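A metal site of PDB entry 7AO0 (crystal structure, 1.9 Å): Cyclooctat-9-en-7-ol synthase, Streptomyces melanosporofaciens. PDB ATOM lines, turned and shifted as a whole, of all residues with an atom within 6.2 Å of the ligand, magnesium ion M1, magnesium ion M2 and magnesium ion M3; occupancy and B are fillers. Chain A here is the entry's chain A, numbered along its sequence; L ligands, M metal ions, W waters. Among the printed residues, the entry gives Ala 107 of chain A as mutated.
Magnesium ion M2 is bound by water W5 (2.1 Å), O4 of the ligand (2.1 Å), water W7 (2.2 Å), O3 of the ligand (2.2 Å), OD2 of Asp 110 (2.3 Å) and water W11 (2.4 Å). Magnesium ion M2 has six donor atoms within binding distance.
Water W2 bridges OD2 of Asp 180 (2.5 Å) and NH1 of Arg 177 (3.3 Å). Water W9 lies within hydrogen-bond range of the side-chain carboxylate (OD1) of Asp 153 and the side-chain carboxylate (OD1) of Asp 180. Water W4 bridges O of Asp 180 (2.6 Å) and O6 of the ligand (2.7 Å). Water W1 bridges the side-chain amide oxygen of Asn 103 (2.7 Å) and a nitrogen (N1) of the ligand (2.7 Å). Water W8 lies within hydrogen-bond range of an oxygen (O1) of the ligand (2.8 Å) and the guanidinium group of Arg 294 (3.2 Å). Water W6 lies within hydrogen-bond range of N1 of the ligand, OG1 of Thr 106, O of Asn 103 and N of Ala 107.
Magnesium ion M1 is bound by OE2 of Glu 228, O2 of the ligand, O5 of the ligand, water W10, OD1 of Asn 220 and OG of Ser 224.
Hydrophobic or aromatic side chains that line the ligand: Ile 181 and Tyr 295. Nine residues have an atom within 4 Å of the ligand: Asp 110, Arg 177, Ile 181, Asn 220, Ser 224, Arg 227, Glu 228, Arg 294 and Tyr 295.
Asp 180 touches magnesium ion M3 (OD2 to MG, 3.98 Å). Two residues have an atom within 4 Å of magnesium ion M3: Asp 110 and Asp 180.
The backbone carbonyl oxygen (O) of Glu 228 sits at hydrogen-bond distance from the backbone NH (N) of Gln 233. OE1 of Glu 228 lies within hydrogen-bond range of ND2 of Asn 236, at 3.1 Å. The side-chain amide nitrogen of Asn 220 sits at hydrogen-bond distance from the side-chain hydroxyl of Tyr 295 (3.2 Å). The guanidinium group (NH1) of Arg 177 lies within salt-bridge range of the side-chain carboxylate (OD2) of Asp 180, at 3.0 Å. NH2 of Arg 177 lies within salt-bridge range of OD1 of Asp 221. The guanidinium group (NH2) of Arg 294 is in salt-bridge range of the side-chain carboxylate (OD1) of Asp 111, 2.8 Å away.
One residue has an atom within 4 Å of magnesium ion M2: Asp 110. The nearest printed residue that does not touch magnesium ion M2 is Arg 294 (4.2 Å).
OH of Tyr 295 lies within hydrogen-bond range of O1 of the ligand (2.5 Å). An oxygen (O6) of the ligand lies within salt-bridge range of the guanidinium group of Arg 177, at 2.7 Å. NH2 of Arg 227 lies within salt-bridge range of O1 of the ligand. The guanidinium group (NE) of Arg 294 lies within salt-bridge range of an oxygen (O1) of the ligand, 2.9 Å away. A nitrogen (N1) of the ligand lies within hydrogen-bond range of the backbone carbonyl oxygen (O) of Ile 181.
OD1 of Asp 110 binds magnesium ion M3, 2.0 Å away. Magnesium ion M3 is bound by water W4 (2.0 Å). O4 of the ligand binds magnesium ion M3, 2.1 Å away. Magnesium ion M3 is bound by water W11 (2.1 Å). Water W2 is bound to magnesium ion M3 (2.1 Å). Water W9 is bound to magnesium ion M3 (2.2 Å). Magnesium ion M3 has six donor atoms within binding distance.
Within 4 Å of magnesium ion M1: Asn 220, Ser 224 and Glu 228.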
ATOM      1  N   ASN A 103      -0.874 -20.879  -3.623  1.00  0.00           N
ATOM      2  CA  ASN A 103      -1.559 -20.333  -4.793  1.00  0.00           C
ATOM      3  C   ASN A 103      -0.750 -20.585  -6.057  1.00  0.00           C
ATOM      4  O   ASN A 103      -1.275 -21.092  -7.063  1.00  0.00           O
ATOM      5  CB  ASN A 103      -1.804 -18.841  -4.590  1.00  0.00           C
ATOM      6  CG  ASN A 103      -2.077 -18.115  -5.893  1.00  0.00           C
ATOM      7  OD1 ASN A 103      -3.217 -18.082  -6.376  1.00  0.00           O
ATOM      8  ND2 ASN A 103      -1.031 -17.527  -6.465  1.00  0.00           N
ATOM      9  N   THR A 106      -0.279 -24.510  -7.113  1.00  0.00           N
ATOM     10  CA  THR A 106      -1.524 -25.062  -7.642  1.00  0.00           C
ATOM     11  C   THR A 106      -2.014 -24.337  -8.878  1.00  0.00           C
ATOM     12  O   THR A 106      -2.822 -24.911  -9.635  1.00  0.00           O
ATOM     13  CB  THR A 106      -2.625 -25.065  -6.579  1.00  0.00           C
ATOM     14  OG1 THR A 106      -2.976 -23.715  -6.207  1.00  0.00           O
ATOM     15  CG2 THR A 106      -2.180 -25.848  -5.354  1.00  0.00           C
ATOM     16  N   ALA A 107      -1.566 -23.104  -9.127  1.00  0.00           N
ATOM     17  CA  ALA A 107      -1.840 -22.468 -10.415  1.00  0.00           C
ATOM     18  C   ALA A 107      -1.069 -23.153 -11.536  1.00  0.00           C
ATOM     19  O   ALA A 107      -1.555 -23.264 -12.664  1.00  0.00           O
ATOM     20  CB  ALA A 107      -1.476 -20.983 -10.366  1.00  0.00           C
ATOM     21  N   ASP A 110      -2.980 -26.135 -12.334  1.00  0.00           N
ATOM     22  CA  ASP A 110      -4.148 -25.764 -13.121  1.00  0.00           C
ATOM     23  C   ASP A 110      -3.787 -25.590 -14.587  1.00  0.00           C
ATOM     24  O   ASP A 110      -4.615 -25.811 -15.467  1.00  0.00           O
ATOM     25  CB  ASP A 110      -4.744 -24.483 -12.545  1.00  0.00           C
ATOM     26  CG  ASP A 110      -5.927 -23.954 -13.341  1.00  0.00           C
ATOM     27  OD1 ASP A 110      -7.058 -24.440 -13.097  1.00  0.00           O
ATOM     28  OD2 ASP A 110      -5.749 -23.001 -14.161  1.00  0.00           O
ATOM     29  N   ASP A 111      -2.543 -25.224 -14.873  1.00  0.00           N
ATOM     30  CA  ASP A 111      -2.110 -25.027 -16.248  1.00  0.00           C
ATOM     31  C   ASP A 111      -1.531 -26.279 -16.884  1.00  0.00           C
ATOM     32  O   ASP A 111      -1.290 -26.284 -18.090  1.00  0.00           O
ATOM     33  CB  ASP A 111      -1.073 -23.879 -16.318  1.00  0.00           C
ATOM     34  CG  ASP A 111      -1.733 -22.518 -16.294  1.00  0.00           C
ATOM     35  OD1 ASP A 111      -2.961 -22.448 -16.567  1.00  0.00           O
ATOM     36  OD2 ASP A 111      -1.053 -21.535 -15.983  1.00  0.00           O
ATOM     37  N   PHE A 149      -8.461 -29.073  -3.939  1.00  0.00           N
ATOM     38  CA  PHE A 149      -8.431 -28.242  -5.146  1.00  0.00           C
ATOM     39  C   PHE A 149      -7.748 -28.964  -6.297  1.00  0.00           C
ATOM     40  O   PHE A 149      -8.261 -28.956  -7.418  1.00  0.00           O
ATOM     41  CB  PHE A 149      -7.720 -26.906  -4.875  1.00  0.00           C
ATOM     42  CG  PHE A 149      -7.580 -26.071  -6.123  1.00  0.00           C
ATOM     43  CD1 PHE A 149      -8.662 -25.372  -6.629  1.00  0.00           C
ATOM     44  CD2 PHE A 149      -6.364 -26.042  -6.821  1.00  0.00           C
ATOM     45  CE1 PHE A 149      -8.550 -24.603  -7.791  1.00  0.00           C
ATOM     46  CE2 PHE A 149      -6.246 -25.278  -7.976  1.00  0.00           C
ATOM     47  CZ  PHE A 149      -7.342 -24.564  -8.472  1.00  0.00           C
ATOM     48  N   ASP A 153      -9.534 -30.180  -9.909  1.00  0.00           N
ATOM     49  CA  ASP A 153      -9.027 -29.780 -11.219  1.00  0.00           C
ATOM     50  C   ASP A 153      -8.714 -31.007 -12.082  1.00  0.00           C
ATOM     51  O   ASP A 153      -9.125 -31.069 -13.242  1.00  0.00           O
ATOM     52  CB  ASP A 153      -7.776 -28.902 -11.045  1.00  0.00           C
ATOM     53  CG  ASP A 153      -7.147 -28.557 -12.370  1.00  0.00           C
ATOM     54  OD1 ASP A 153      -7.851 -28.003 -13.244  1.00  0.00           O
ATOM     55  OD2 ASP A 153      -5.963 -28.893 -12.554  1.00  0.00           O
ATOM     56  N   ARG A 177     -17.939 -23.519  -9.616  1.00  0.00           N
ATOM     57  CA  ARG A 177     -16.774 -22.655  -9.421  1.00  0.00           C
ATOM     58  C   ARG A 177     -16.403 -22.432  -7.952  1.00  0.00           C
ATOM     59  O   ARG A 177     -15.264 -22.054  -7.690  1.00  0.00           O
ATOM     60  CB  ARG A 177     -17.018 -21.314 -10.115  1.00  0.00           C
ATOM     61  CG  ARG A 177     -16.981 -21.472 -11.630  1.00  0.00           C
ATOM     62  CD  ARG A 177     -15.576 -21.906 -12.093  1.00  0.00           C
ATOM     63  NE  ARG A 177     -14.948 -20.820 -12.845  1.00  0.00           N
ATOM     64  CZ  ARG A 177     -13.638 -20.644 -12.996  1.00  0.00           C
ATOM     65  NH1 ARG A 177     -12.763 -21.464 -12.449  1.00  0.00           N
ATOM     66  NH2 ARG A 177     -13.209 -19.606 -13.708  1.00  0.00           N
ATOM     67  N   ASP A 180     -13.913 -25.018  -8.018  1.00  0.00           N
ATOM     68  CA  ASP A 180     -12.997 -25.058  -9.160  1.00  0.00           C
ATOM     69  C   ASP A 180     -12.147 -23.789  -9.294  1.00  0.00           C
ATOM     70  O   ASP A 180     -10.979 -23.868  -9.668  1.00  0.00           O
ATOM     71  CB  ASP A 180     -13.769 -25.289 -10.453  1.00  0.00           C
ATOM     72  CG  ASP A 180     -12.854 -25.408 -11.662  1.00  0.00           C
ATOM     73  OD1 ASP A 180     -12.239 -26.476 -11.884  1.00  0.00           O
ATOM     74  OD2 ASP A 180     -12.754 -24.417 -12.426  1.00  0.00           O
ATOM     75  N   ILE A 181     -12.715 -22.618  -9.024  1.00  0.00           N
ATOM     76  CA  ILE A 181     -11.889 -21.420  -9.153  1.00  0.00           C
ATOM     77  C   ILE A 181     -10.863 -21.323  -8.031  1.00  0.00           C
ATOM     78  O   ILE A 181      -9.897 -20.562  -8.146  1.00  0.00           O
ATOM     79  CB  ILE A 181     -12.730 -20.140  -9.246  1.00  0.00           C
ATOM     80  CG1 ILE A 181     -11.860 -19.011  -9.808  1.00  0.00           C
ATOM     81  CG2 ILE A 181     -13.331 -19.715  -7.892  1.00  0.00           C
ATOM     82  CD1 ILE A 181     -12.612 -17.869 -10.411  1.00  0.00           C
ATOM     83  N   GLY A 182     -11.017 -22.118  -6.983  1.00  0.00           N
ATOM     84  CA  GLY A 182     -10.067 -22.107  -5.894  1.00  0.00           C
ATOM     85  C   GLY A 182     -10.414 -21.228  -4.713  1.00  0.00           C
ATOM     86  O   GLY A 182      -9.600 -21.132  -3.780  1.00  0.00           O
ATOM     87  N   ASN A 220     -12.661 -12.939 -13.511  1.00  0.00           N
ATOM     88  CA  ASN A 220     -11.679 -13.803 -14.146  1.00  0.00           C
ATOM     89  C   ASN A 220     -12.189 -14.333 -15.476  1.00  0.00           C
ATOM     90  O   ASN A 220     -11.447 -14.393 -16.461  1.00  0.00           O
ATOM     91  CB  ASN A 220     -11.285 -14.963 -13.233  1.00  0.00           C
ATOM     92  CG  ASN A 220     -10.394 -15.930 -13.970  1.00  0.00           C
ATOM     93  OD1 ASN A 220     -10.847 -16.933 -14.467  1.00  0.00           O
ATOM     94  ND2 ASN A 220      -9.110 -15.558 -14.121  1.00  0.00           N
ATOM     95  N   ASP A 221     -13.462 -14.702 -15.531  1.00  0.00           N
ATOM     96  CA  ASP A 221     -13.961 -15.289 -16.762  1.00  0.00           C
ATOM     97  C   ASP A 221     -13.875 -14.296 -17.915  1.00  0.00           C
ATOM     98  O   ASP A 221     -13.586 -14.675 -19.049  1.00  0.00           O
ATOM     99  CB  ASP A 221     -15.391 -15.773 -16.599  1.00  0.00           C
ATOM    100  CG  ASP A 221     -15.475 -17.010 -15.724  1.00  0.00           C
ATOM    101  OD1 ASP A 221     -14.397 -17.535 -15.369  1.00  0.00           O
ATOM    102  OD2 ASP A 221     -16.607 -17.441 -15.414  1.00  0.00           O
ATOM    103  N   SER A 224     -10.158 -14.000 -18.990  1.00  0.00           N
ATOM    104  CA  SER A 224      -9.504 -15.224 -19.426  1.00  0.00           C
ATOM    105  C   SER A 224     -10.283 -15.923 -20.555  1.00  0.00           C
ATOM    106  O   SER A 224      -9.847 -16.980 -21.032  1.00  0.00           O
ATOM    107  CB  SER A 224      -9.294 -16.171 -18.234  1.00  0.00           C
ATOM    108  OG  SER A 224     -10.504 -16.414 -17.511  1.00  0.00           O
ATOM    109  N   TYR A 225     -11.386 -15.332 -21.020  1.00  0.00           N
ATOM    110  CA  TYR A 225     -12.214 -15.954 -22.042  1.00  0.00           C
ATOM    111  C   TYR A 225     -11.407 -16.272 -23.306  1.00  0.00           C
ATOM    112  O   TYR A 225     -11.398 -17.414 -23.784  1.00  0.00           O
ATOM    113  CB  TYR A 225     -13.397 -15.035 -22.347  1.00  0.00           C
ATOM    114  CG  TYR A 225     -14.358 -15.581 -23.358  1.00  0.00           C
ATOM    115  CD1 TYR A 225     -14.128 -15.407 -24.721  1.00  0.00           C
ATOM    116  CD2 TYR A 225     -15.468 -16.308 -22.969  1.00  0.00           C
ATOM    117  CE1 TYR A 225     -14.979 -15.927 -25.663  1.00  0.00           C
ATOM    118  CE2 TYR A 225     -16.343 -16.834 -23.905  1.00  0.00           C
ATOM    119  CZ  TYR A 225     -16.078 -16.623 -25.261  1.00  0.00           C
ATOM    120  OH  TYR A 225     -16.917 -17.127 -26.207  1.00  0.00           O
ATOM    121  N   ARG A 227      -8.174 -16.672 -23.937  1.00  0.00           N
ATOM    122  CA  ARG A 227      -7.226 -17.769 -23.730  1.00  0.00           C
ATOM    123  C   ARG A 227      -7.945 -19.105 -23.562  1.00  0.00           C
ATOM    124  O   ARG A 227      -7.566 -20.114 -24.178  1.00  0.00           O
ATOM    125  CB  ARG A 227      -6.352 -17.493 -22.504  1.00  0.00           C
ATOM    126  CG  ARG A 227      -5.620 -18.742 -21.984  1.00  0.00           C
ATOM    127  CD  ARG A 227      -4.546 -18.421 -20.944  1.00  0.00           C
ATOM    128  NE  ARG A 227      -5.107 -17.770 -19.750  1.00  0.00           N
ATOM    129  CZ  ARG A 227      -5.782 -18.399 -18.787  1.00  0.00           C
ATOM    130  NH1 ARG A 227      -5.998 -19.703 -18.827  1.00  0.00           N
ATOM    131  NH2 ARG A 227      -6.263 -17.713 -17.750  1.00  0.00           N
ATOM    132  N   GLU A 228      -8.984 -19.139 -22.725  1.00  0.00           N
ATOM    133  CA  GLU A 228      -9.642 -20.410 -22.434  1.00  0.00           C
ATOM    134  C   GLU A 228     -10.324 -20.974 -23.672  1.00  0.00           C
ATOM    135  O   GLU A 228     -10.182 -22.169 -23.963  1.00  0.00           O
ATOM    136  CB  GLU A 228     -10.616 -20.207 -21.261  1.00  0.00           C
ATOM    137  CG  GLU A 228      -9.812 -20.029 -19.961  1.00  0.00           C
ATOM    138  CD  GLU A 228     -10.625 -19.638 -18.753  1.00  0.00           C
ATOM    139  OE1 GLU A 228     -11.858 -19.417 -18.893  1.00  0.00           O
ATOM    140  OE2 GLU A 228     -10.001 -19.547 -17.665  1.00  0.00           O
ATOM    141  N   GLN A 233     -11.083 -24.861 -23.277  1.00  0.00           N
ATOM    142  CA  GLN A 233     -11.540 -24.898 -21.881  1.00  0.00           C
ATOM    143  C   GLN A 233     -12.965 -24.332 -21.783  1.00  0.00           C
ATOM    144  O   GLN A 233     -13.235 -23.236 -22.276  1.00  0.00           O
ATOM    145  CB  GLN A 233     -10.569 -24.117 -20.987  1.00  0.00           C
ATOM    146  CG  GLN A 233      -9.212 -24.829 -20.896  1.00  0.00           C
ATOM    147  CD  GLN A 233      -8.171 -24.041 -20.134  1.00  0.00           C
ATOM    148  OE1 GLN A 233      -7.818 -22.940 -20.522  1.00  0.00           O
ATOM    149  NE2 GLN A 233      -7.661 -24.611 -19.040  1.00  0.00           N
ATOM    150  N   THR A 235     -14.852 -23.899 -18.900  1.00  0.00           N
ATOM    151  CA  THR A 235     -15.251 -23.414 -17.579  1.00  0.00           C
ATOM    152  C   THR A 235     -15.173 -21.883 -17.591  1.00  0.00           C
ATOM    153  O   THR A 235     -14.219 -21.271 -17.087  1.00  0.00           O
ATOM    154  CB  THR A 235     -14.347 -24.036 -16.506  1.00  0.00           C
ATOM    155  OG1 THR A 235     -14.351 -25.471 -16.627  1.00  0.00           O
ATOM    156  CG2 THR A 235     -14.819 -23.674 -15.111  1.00  0.00           C
ATOM    157  N   ASN A 236     -16.179 -21.255 -18.196  1.00  0.00           N
ATOM    158  CA  ASN A 236     -16.228 -19.794 -18.310  1.00  0.00           C
ATOM    159  C   ASN A 236     -17.673 -19.383 -18.550  1.00  0.00           C
ATOM    160  O   ASN A 236     -18.286 -19.847 -19.520  1.00  0.00           O
ATOM    161  CB  ASN A 236     -15.350 -19.338 -19.468  1.00  0.00           C
ATOM    162  CG  ASN A 236     -15.240 -17.823 -19.568  1.00  0.00           C
ATOM    163  OD1 ASN A 236     -16.248 -17.104 -19.648  1.00  0.00           O
ATOM    164  ND2 ASN A 236     -13.994 -17.326 -19.585  1.00  0.00           N
ATOM    165  N   ARG A 294      -0.811 -12.353 -18.389  1.00  0.00           N
ATOM    166  CA  ARG A 294      -1.513 -13.625 -18.632  1.00  0.00           C
ATOM    167  C   ARG A 294      -2.858 -13.401 -19.312  1.00  0.00           C
ATOM    168  O   ARG A 294      -3.233 -14.140 -20.232  1.00  0.00           O
ATOM    169  CB  ARG A 294      -1.693 -14.384 -17.308  1.00  0.00           C
ATOM    170  CG  ARG A 294      -2.688 -15.571 -17.394  1.00  0.00           C
ATOM    171  CD  ARG A 294      -2.863 -16.265 -16.056  1.00  0.00           C
ATOM    172  NE  ARG A 294      -3.641 -17.505 -16.129  1.00  0.00           N
ATOM    173  CZ  ARG A 294      -3.114 -18.719 -16.331  1.00  0.00           C
ATOM    174  NH1 ARG A 294      -1.810 -18.838 -16.513  1.00  0.00           N
ATOM    175  NH2 ARG A 294      -3.890 -19.802 -16.344  1.00  0.00           N
ATOM    176  N   TYR A 295      -3.599 -12.386 -18.893  1.00  0.00           N
ATOM    177  CA  TYR A 295      -4.952 -12.129 -19.374  1.00  0.00           C
ATOM    178  C   TYR A 295      -4.992 -11.101 -20.490  1.00  0.00           C
ATOM    179  O   TYR A 295      -5.960 -10.341 -20.601  1.00  0.00           O
ATOM    180  CB  TYR A 295      -5.837 -11.673 -18.221  1.00  0.00           C
ATOM    181  CG  TYR A 295      -5.872 -12.660 -17.087  1.00  0.00           C
ATOM    182  CD1 TYR A 295      -6.237 -13.980 -17.317  1.00  0.00           C
ATOM    183  CD2 TYR A 295      -5.518 -12.286 -15.809  1.00  0.00           C
ATOM    184  CE1 TYR A 295      -6.263 -14.912 -16.272  1.00  0.00           C
ATOM    185  CE2 TYR A 295      -5.542 -13.206 -14.757  1.00  0.00           C
ATOM    186  CZ  TYR A 295      -5.913 -14.509 -15.000  1.00  0.00           C
ATOM    187  OH  TYR A 295      -5.931 -15.414 -13.978  1.00  0.00           O
HETATM  188  C1  LIG L   1      -7.286 -19.968 -10.982  1.00  0.00           C
HETATM  189  C2  LIG L   1      -6.536 -20.891 -10.014  1.00  0.00           C
HETATM  190  C3  LIG L   1      -6.900 -20.203 -12.451  1.00  0.00           C
HETATM  191  C4  LIG L   1      -7.917 -19.422 -13.269  1.00  0.00           C
HETATM  192  O1  LIG L   1      -5.980 -17.870 -14.533  1.00  0.00           O
HETATM  193  P1  LIG L   1      -7.159 -18.807 -14.827  1.00  0.00           P
HETATM  194  O2  LIG L   1      -8.152 -18.053 -15.681  1.00  0.00           O
HETATM  195  O3  LIG L   1      -6.661 -20.027 -15.516  1.00  0.00           O
HETATM  196  P2  LIG L   1      -9.330 -20.566 -13.669  1.00  0.00           P
HETATM  197  O4  LIG L   1      -8.733 -21.894 -14.070  1.00  0.00           O
HETATM  198  O5  LIG L   1     -10.121 -20.027 -14.805  1.00  0.00           O
HETATM  199  O6  LIG L   1     -10.154 -20.714 -12.405  1.00  0.00           O
HETATM  200  O7  LIG L   1      -8.378 -18.353 -12.503  1.00  0.00           O
HETATM  201  N1  LIG L   1      -6.797 -20.462  -8.639  1.00  0.00           N
HETATM  202 MG    MG M   1     -10.194 -18.299 -16.038  1.00  0.00          MG
HETATM  203 MG    MG M   2      -7.294 -22.090 -15.550  1.00  0.00          MG
HETATM  204 MG    MG M   3      -8.944 -23.880 -13.427  1.00  0.00          MG
HETATM  205  O   HOH W   1      -4.705 -18.824  -8.448  1.00  0.00           O
HETATM  206  O   HOH W   2     -11.001 -23.817 -14.039  1.00  0.00           O
HETATM  207  O   HOH W   3     -11.759 -21.798 -16.051  1.00  0.00           O
HETATM  208  O   HOH W   4      -9.356 -23.140 -11.606  1.00  0.00           O
HETATM  209  O   HOH W   5      -8.278 -21.616 -17.310  1.00  0.00           O
HETATM  210  O   HOH W   6      -4.260 -21.688  -7.896  1.00  0.00           O
HETATM  211  O   HOH W   7      -5.819 -22.611 -17.027  1.00  0.00           O
HETATM  212  O   HOH W   8      -3.666 -18.616 -13.079  1.00  0.00           O
HETATM  213  O   HOH W   9      -9.464 -25.908 -12.782  1.00  0.00           O
HETATM  214  O   HOH W  10     -12.295 -18.577 -16.476  1.00  0.00           O
HETATM  215  O   HOH W  11      -8.404 -24.162 -15.477  1.00  0.00           O
